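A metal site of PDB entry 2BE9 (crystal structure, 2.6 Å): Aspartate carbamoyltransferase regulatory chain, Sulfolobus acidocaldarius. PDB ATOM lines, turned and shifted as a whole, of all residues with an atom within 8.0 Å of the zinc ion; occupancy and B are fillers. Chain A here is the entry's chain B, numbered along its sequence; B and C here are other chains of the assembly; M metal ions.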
ATOM      1  N   LYS A 116      27.170 -19.698 -25.570  1.00  0.00           N
ATOM      2  CA  LYS A 116      27.568 -18.778 -24.516  1.00  0.00           C
ATOM      3  C   LYS A 116      26.534 -17.650 -24.328  1.00  0.00           C
ATOM      4  O   LYS A 116      25.749 -17.355 -25.217  1.00  0.00           O
ATOM      5  CB  LYS A 116      28.931 -18.166 -24.843  1.00  0.00           C
ATOM      6  CG  LYS A 116      30.123 -19.073 -24.585  1.00  0.00           C
ATOM      7  CD  LYS A 116      31.436 -18.372 -25.032  1.00  0.00           C
ATOM      8  CE  LYS A 116      32.672 -19.195 -24.705  1.00  0.00           C
ATOM      9  NZ  LYS A 116      33.855 -18.705 -25.480  1.00  0.00           N
ATOM     10  N   CYS A 117      26.548 -17.024 -23.153  1.00  0.00           N
ATOM     11  CA  CYS A 117      25.639 -15.915 -22.899  1.00  0.00           C
ATOM     12  C   CYS A 117      26.304 -14.601 -23.281  1.00  0.00           C
ATOM     13  O   CYS A 117      27.424 -14.303 -22.818  1.00  0.00           O
ATOM     14  CB  CYS A 117      25.187 -15.915 -21.427  1.00  0.00           C
ATOM     15  SG  CYS A 117      23.918 -14.672 -21.000  1.00  0.00           S
ATOM     16  N   PRO A 118      25.645 -13.813 -24.147  1.00  0.00           N
ATOM     17  CA  PRO A 118      26.223 -12.507 -24.535  1.00  0.00           C
ATOM     18  C   PRO A 118      26.318 -11.503 -23.385  1.00  0.00           C
ATOM     19  O   PRO A 118      27.050 -10.533 -23.506  1.00  0.00           O
ATOM     20  CB  PRO A 118      25.263 -11.985 -25.615  1.00  0.00           C
ATOM     21  CG  PRO A 118      24.008 -12.764 -25.452  1.00  0.00           C
ATOM     22  CD  PRO A 118      24.353 -14.080 -24.805  1.00  0.00           C
ATOM     23  N   ASN A 119      25.609 -11.712 -22.279  1.00  0.00           N
ATOM     24  CA  ASN A 119      25.721 -10.813 -21.120  1.00  0.00           C
ATOM     25  C   ASN A 119      27.075 -10.965 -20.401  1.00  0.00           C
ATOM     26  O   ASN A 119      27.328 -11.962 -19.750  1.00  0.00           O
ATOM     27  CB  ASN A 119      24.534 -10.982 -20.165  1.00  0.00           C
ATOM     28  CG  ASN A 119      24.732 -10.241 -18.827  1.00  0.00           C
ATOM     29  OD1 ASN A 119      25.535  -9.313 -18.728  1.00  0.00           O
ATOM     30  ND2 ASN A 119      23.990 -10.656 -17.808  1.00  0.00           N
ATOM     31  N   PRO A 120      27.955  -9.948 -20.507  1.00  0.00           N
ATOM     32  CA  PRO A 120      29.269 -10.072 -19.876  1.00  0.00           C
ATOM     33  C   PRO A 120      29.174 -10.206 -18.350  1.00  0.00           C
ATOM     34  O   PRO A 120      30.116 -10.680 -17.722  1.00  0.00           O
ATOM     35  CB  PRO A 120      29.971  -8.767 -20.254  1.00  0.00           C
ATOM     36  CG  PRO A 120      28.865  -7.809 -20.533  1.00  0.00           C
ATOM     37  CD  PRO A 120      27.812  -8.627 -21.173  1.00  0.00           C
ATOM     38  N   TYR A 121      28.032  -9.814 -17.781  1.00  0.00           N
ATOM     39  CA  TYR A 121      27.794  -9.877 -16.339  1.00  0.00           C
ATOM     40  C   TYR A 121      27.107 -11.151 -15.890  1.00  0.00           C
ATOM     41  O   TYR A 121      26.949 -11.369 -14.701  1.00  0.00           O
ATOM     42  CB  TYR A 121      26.991  -8.658 -15.879  1.00  0.00           C
ATOM     43  CG  TYR A 121      27.796  -7.409 -16.027  1.00  0.00           C
ATOM     44  CD1 TYR A 121      27.622  -6.571 -17.138  1.00  0.00           C
ATOM     45  CD2 TYR A 121      28.799  -7.092 -15.098  1.00  0.00           C
ATOM     46  CE1 TYR A 121      28.399  -5.451 -17.294  1.00  0.00           C
ATOM     47  CE2 TYR A 121      29.571  -5.976 -15.247  1.00  0.00           C
ATOM     48  CZ  TYR A 121      29.371  -5.162 -16.349  1.00  0.00           C
ATOM     49  OH  TYR A 121      30.145  -4.047 -16.484  1.00  0.00           O
ATOM     50  N   CYS A 122      26.722 -11.992 -16.843  1.00  0.00           N
ATOM     51  CA  CYS A 122      26.153 -13.281 -16.520  1.00  0.00           C
ATOM     52  C   CYS A 122      27.188 -14.111 -15.797  1.00  0.00           C
ATOM     53  O   CYS A 122      28.350 -14.158 -16.209  1.00  0.00           O
ATOM     54  CB  CYS A 122      25.724 -14.020 -17.772  1.00  0.00           C
ATOM     55  SG  CYS A 122      24.754 -15.505 -17.408  1.00  0.00           S
ATOM     56  N   ILE A 123      26.761 -14.750 -14.716  1.00  0.00           N
ATOM     57  CA  ILE A 123      27.602 -15.658 -13.977  1.00  0.00           C
ATOM     58  C   ILE A 123      28.238 -16.746 -14.886  1.00  0.00           C
ATOM     59  O   ILE A 123      29.415 -17.114 -14.690  1.00  0.00           O
ATOM     60  CB  ILE A 123      26.824 -16.308 -12.798  1.00  0.00           C
ATOM     61  CG1 ILE A 123      27.751 -17.154 -11.937  1.00  0.00           C
ATOM     62  CG2 ILE A 123      25.599 -17.079 -13.299  1.00  0.00           C
ATOM     63  CD1 ILE A 123      28.769 -16.353 -11.181  1.00  0.00           C
ATOM     64  N   THR A 124      27.490 -17.219 -15.879  1.00  0.00           N
ATOM     65  CA  THR A 124      28.009 -18.188 -16.852  1.00  0.00           C
ATOM     66  C   THR A 124      29.141 -17.637 -17.727  1.00  0.00           C
ATOM     67  O   THR A 124      29.851 -18.423 -18.379  1.00  0.00           O
ATOM     68  CB  THR A 124      26.872 -18.800 -17.734  1.00  0.00           C
ATOM     69  OG1 THR A 124      26.353 -17.809 -18.622  1.00  0.00           O
ATOM     70  CG2 THR A 124      25.721 -19.341 -16.864  1.00  0.00           C
ATOM     71  N   SER A 125      29.314 -16.313 -17.748  1.00  0.00           N
ATOM     72  CA  SER A 125      30.398 -15.656 -18.516  1.00  0.00           C
ATOM     73  C   SER A 125      31.631 -15.412 -17.640  1.00  0.00           C
ATOM     74  O   SER A 125      32.577 -14.753 -18.074  1.00  0.00           O
ATOM     75  CB  SER A 125      29.965 -14.295 -19.054  1.00  0.00           C
ATOM     76  OG  SER A 125      28.866 -14.382 -19.932  1.00  0.00           O
ATOM     77  N   PRO A 132      26.988 -22.277 -19.294  1.00  0.00           N
ATOM     78  CA  PRO A 132      25.911 -21.579 -19.995  1.00  0.00           C
ATOM     79  C   PRO A 132      24.720 -22.502 -20.305  1.00  0.00           C
ATOM     80  O   PRO A 132      24.911 -23.644 -20.732  1.00  0.00           O
ATOM     81  CB  PRO A 132      26.573 -21.085 -21.281  1.00  0.00           C
ATOM     82  CG  PRO A 132      28.059 -21.012 -20.953  1.00  0.00           C
ATOM     83  CD  PRO A 132      28.312 -22.052 -19.912  1.00  0.00           C
ATOM     84  N   THR A 133      23.505 -22.014 -20.082  1.00  0.00           N
ATOM     85  CA  THR A 133      22.322 -22.844 -20.205  1.00  0.00           C
ATOM     86  C   THR A 133      21.179 -22.007 -20.761  1.00  0.00           C
ATOM     87  O   THR A 133      20.812 -20.995 -20.178  1.00  0.00           O
ATOM     88  CB  THR A 133      21.932 -23.470 -18.835  1.00  0.00           C
ATOM     89  OG1 THR A 133      23.032 -24.243 -18.359  1.00  0.00           O
ATOM     90  CG2 THR A 133      20.705 -24.367 -18.949  1.00  0.00           C
ATOM     91  N   PHE A 134      20.632 -22.451 -21.879  1.00  0.00           N
ATOM     92  CA  PHE A 134      19.545 -21.727 -22.529  1.00  0.00           C
ATOM     93  C   PHE A 134      18.322 -22.607 -22.643  1.00  0.00           C
ATOM     94  O   PHE A 134      18.417 -23.793 -22.956  1.00  0.00           O
ATOM     95  CB  PHE A 134      20.005 -21.148 -23.885  1.00  0.00           C
ATOM     96  CG  PHE A 134      20.835 -19.894 -23.759  1.00  0.00           C
ATOM     97  CD1 PHE A 134      22.191 -19.962 -23.429  1.00  0.00           C
ATOM     98  CD2 PHE A 134      20.246 -18.634 -23.908  1.00  0.00           C
ATOM     99  CE1 PHE A 134      22.945 -18.791 -23.269  1.00  0.00           C
ATOM    100  CE2 PHE A 134      21.011 -17.466 -23.756  1.00  0.00           C
ATOM    101  CZ  PHE A 134      22.350 -17.547 -23.432  1.00  0.00           C
ATOM    102  N   ARG A 145      16.353 -18.353 -24.009  1.00  0.00           N
ATOM    103  CA  ARG A 145      16.531 -17.518 -22.837  1.00  0.00           C
ATOM    104  C   ARG A 145      17.579 -18.108 -21.896  1.00  0.00           C
ATOM    105  O   ARG A 145      17.479 -19.274 -21.536  1.00  0.00           O
ATOM    106  CB  ARG A 145      15.209 -17.422 -22.089  1.00  0.00           C
ATOM    107  CG  ARG A 145      14.976 -16.086 -21.453  1.00  0.00           C
ATOM    108  CD  ARG A 145      14.537 -16.243 -20.022  1.00  0.00           C
ATOM    109  NE  ARG A 145      13.223 -16.883 -19.886  1.00  0.00           N
ATOM    110  CZ  ARG A 145      13.007 -18.022 -19.244  1.00  0.00           C
ATOM    111  NH1 ARG A 145      11.769 -18.496 -19.167  1.00  0.00           N
ATOM    112  NH2 ARG A 145      14.013 -18.702 -18.657  1.00  0.00           N
ATOM    113  N   CYS A 146      18.573 -17.311 -21.521  1.00  0.00           N
ATOM    114  CA  CYS A 146      19.573 -17.724 -20.520  1.00  0.00           C
ATOM    115  C   CYS A 146      18.897 -17.983 -19.183  1.00  0.00           C
ATOM    116  O   CYS A 146      18.175 -17.111 -18.684  1.00  0.00           O
ATOM    117  CB  CYS A 146      20.645 -16.635 -20.365  1.00  0.00           C
ATOM    118  SG  CYS A 146      21.784 -16.846 -19.009  1.00  0.00           S
ATOM    119  N   GLU A 147      19.126 -19.152 -18.606  1.00  0.00           N
ATOM    120  CA  GLU A 147      18.425 -19.542 -17.370  1.00  0.00           C
ATOM    121  C   GLU A 147      18.927 -18.833 -16.119  1.00  0.00           C
ATOM    122  O   GLU A 147      18.293 -18.905 -15.065  1.00  0.00           O
ATOM    123  CB  GLU A 147      18.511 -21.037 -17.137  1.00  0.00           C
ATOM    124  CG  GLU A 147      17.753 -21.888 -18.168  1.00  0.00           C
ATOM    125  CD  GLU A 147      17.636 -23.329 -17.729  1.00  0.00           C
ATOM    126  OE1 GLU A 147      18.044 -23.624 -16.562  1.00  0.00           O
ATOM    127  OE2 GLU A 147      17.148 -24.157 -18.523  1.00  0.00           O
ATOM    128  N   TYR A 148      20.062 -18.150 -16.244  1.00  0.00           N
ATOM    129  CA  TYR A 148      20.661 -17.463 -15.110  1.00  0.00           C
ATOM    130  C   TYR A 148      20.294 -15.990 -15.075  1.00  0.00           C
ATOM    131  O   TYR A 148      19.910 -15.470 -14.028  1.00  0.00           O
ATOM    132  CB  TYR A 148      22.173 -17.650 -15.111  1.00  0.00           C
ATOM    133  CG  TYR A 148      22.543 -19.077 -14.818  1.00  0.00           C
ATOM    134  CD1 TYR A 148      22.730 -19.515 -13.491  1.00  0.00           C
ATOM    135  CD2 TYR A 148      22.672 -20.006 -15.858  1.00  0.00           C
ATOM    136  CE1 TYR A 148      23.054 -20.836 -13.197  1.00  0.00           C
ATOM    137  CE2 TYR A 148      22.984 -21.336 -15.578  1.00  0.00           C
ATOM    138  CZ  TYR A 148      23.175 -21.745 -14.244  1.00  0.00           C
ATOM    139  OH  TYR A 148      23.484 -23.051 -13.962  1.00  0.00           O
ATOM    140  N   CYS A 149      20.391 -15.325 -16.224  1.00  0.00           N
ATOM    141  CA  CYS A 149      20.233 -13.873 -16.274  1.00  0.00           C
ATOM    142  C   CYS A 149      19.066 -13.420 -17.151  1.00  0.00           C
ATOM    143  O   CYS A 149      18.777 -12.227 -17.210  1.00  0.00           O
ATOM    144  CB  CYS A 149      21.536 -13.217 -16.757  1.00  0.00           C
ATOM    145  SG  CYS A 149      21.819 -13.317 -18.521  1.00  0.00           S
ATOM    146  N   GLU A 150      18.397 -14.366 -17.824  1.00  0.00           N
ATOM    147  CA  GLU A 150      17.200 -14.054 -18.624  1.00  0.00           C
ATOM    148  C   GLU A 150      17.486 -13.350 -19.953  1.00  0.00           C
ATOM    149  O   GLU A 150      16.544 -12.911 -20.618  1.00  0.00           O
ATOM    150  CB  GLU A 150      16.132 -13.236 -17.837  1.00  0.00           C
ATOM    151  CG  GLU A 150      15.849 -13.621 -16.364  1.00  0.00           C
ATOM    152  CD  GLU A 150      15.539 -15.098 -16.163  1.00  0.00           C
ATOM    153  OE1 GLU A 150      15.794 -15.599 -15.051  1.00  0.00           O
ATOM    154  OE2 GLU A 150      15.033 -15.755 -17.086  1.00  0.00           O
ATOM    155  N   THR A 151      18.749 -13.220 -20.334  1.00  0.00           N
ATOM    156  CA  THR A 151      19.057 -12.669 -21.655  1.00  0.00           C
ATOM    157  C   THR A 151      18.496 -13.567 -22.757  1.00  0.00           C
ATOM    158  O   THR A 151      18.552 -14.805 -22.670  1.00  0.00           O
ATOM    159  CB  THR A 151      20.580 -12.454 -21.845  1.00  0.00           C
ATOM    160  OG1 THR A 151      21.051 -11.557 -20.841  1.00  0.00           O
ATOM    161  CG2 THR A 151      20.898 -11.864 -23.202  1.00  0.00           C
ATOM    162  N   ILE A 152      17.952 -12.926 -23.795  1.00  0.00           N
ATOM    163  CA  ILE A 152      17.329 -13.637 -24.907  1.00  0.00           C
ATOM    164  C   ILE A 152      18.253 -13.628 -26.118  1.00  0.00           C
ATOM    165  O   ILE A 152      18.838 -12.603 -26.443  1.00  0.00           O
ATOM    166  CB  ILE A 152      15.966 -12.996 -25.298  1.00  0.00           C
ATOM    167  CG1 ILE A 152      14.954 -13.103 -24.137  1.00  0.00           C
ATOM    168  CG2 ILE A 152      15.400 -13.625 -26.576  1.00  0.00           C
ATOM    169  CD1 ILE A 152      13.560 -12.639 -24.502  1.00  0.00           C
ATOM    170  N   ASP B 106      24.851 -11.437 -12.697  1.00  0.00           N
ATOM    171  CA  ASP B 106      23.482 -11.949 -12.821  1.00  0.00           C
ATOM    172  C   ASP B 106      23.494 -13.473 -12.788  1.00  0.00           C
ATOM    173  O   ASP B 106      24.302 -14.104 -13.466  1.00  0.00           O
ATOM    174  CB  ASP B 106      22.814 -11.520 -14.131  1.00  0.00           C
ATOM    175  CG  ASP B 106      22.880 -10.038 -14.372  1.00  0.00           C
ATOM    176  OD1 ASP B 106      22.467  -9.242 -13.528  1.00  0.00           O
ATOM    177  OD2 ASP B 106      23.322  -9.663 -15.470  1.00  0.00           O
ATOM    178  N   GLY B 107      22.595 -14.026 -11.985  1.00  0.00           N
ATOM    179  CA  GLY B 107      22.418 -15.469 -11.896  1.00  0.00           C
ATOM    180  C   GLY B 107      23.352 -16.074 -10.873  1.00  0.00           C
ATOM    181  O   GLY B 107      23.443 -17.308 -10.789  1.00  0.00           O
ATOM    182  N   MET C 232      26.345  -4.758 -24.233  1.00  0.00           N
ATOM    183  CA  MET C 232      25.661  -5.710 -25.083  1.00  0.00           C
ATOM    184  C   MET C 232      25.086  -5.096 -26.361  1.00  0.00           C
ATOM    185  O   MET C 232      25.106  -5.719 -27.418  1.00  0.00           O
ATOM    186  CB  MET C 232      24.532  -6.381 -24.311  1.00  0.00           C
ATOM    187  CG  MET C 232      24.952  -7.444 -23.316  1.00  0.00           C
ATOM    188  SD  MET C 232      23.509  -8.310 -22.641  1.00  0.00           S
ATOM    189  CE  MET C 232      22.854  -9.059 -24.134  1.00  0.00           C
HETATM  190 ZN    ZN M   1      23.156 -15.229 -18.981  1.00  0.00          ZN
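ND2 of Asn 119 sits close to N of Cys 122 (3.2 Å). The side-chain sulfur (SG) of Cys 149 sits close to the side-chain amide nitrogen (ND2) of Asn 119, at 3.5 Å. OG of Ser 125 is in hydrogen-bond range of O of Cys 117, at 3.2 Å. N of Cys 146 sits at hydrogen-bond distance from O of Thr 151 (2.8 Å). The side-chain hydroxyl (OG1) of Thr 124 lies close to the side-chain sulfur (SG) of Cys 122, 3.1 Å away. The side-chain sulfur (SG) of Cys 149 lies close to the side-chain hydroxyl (OG1) of Thr 151, 3.0 Å away. SG of Cys 146 sits close to N of Tyr 148 (3.5 Å). The backbone NH (N) of Asn 119 lies close to the side-chain sulfur (SG) of Cys 117, at 3.6 Å.
The side-chain sulfur (SG) of Cys 146 binds the zinc ion, 2.1 Å away. The side-chain sulfur (SG) of Cys 117 binds the zinc ion (2.2 Å). The zinc ion is bound by the side-chain sulfur (SG) of Cys 122 (2.3 Å). The zinc ion is bound by the side-chain sulfur (SG) of Cys 149.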
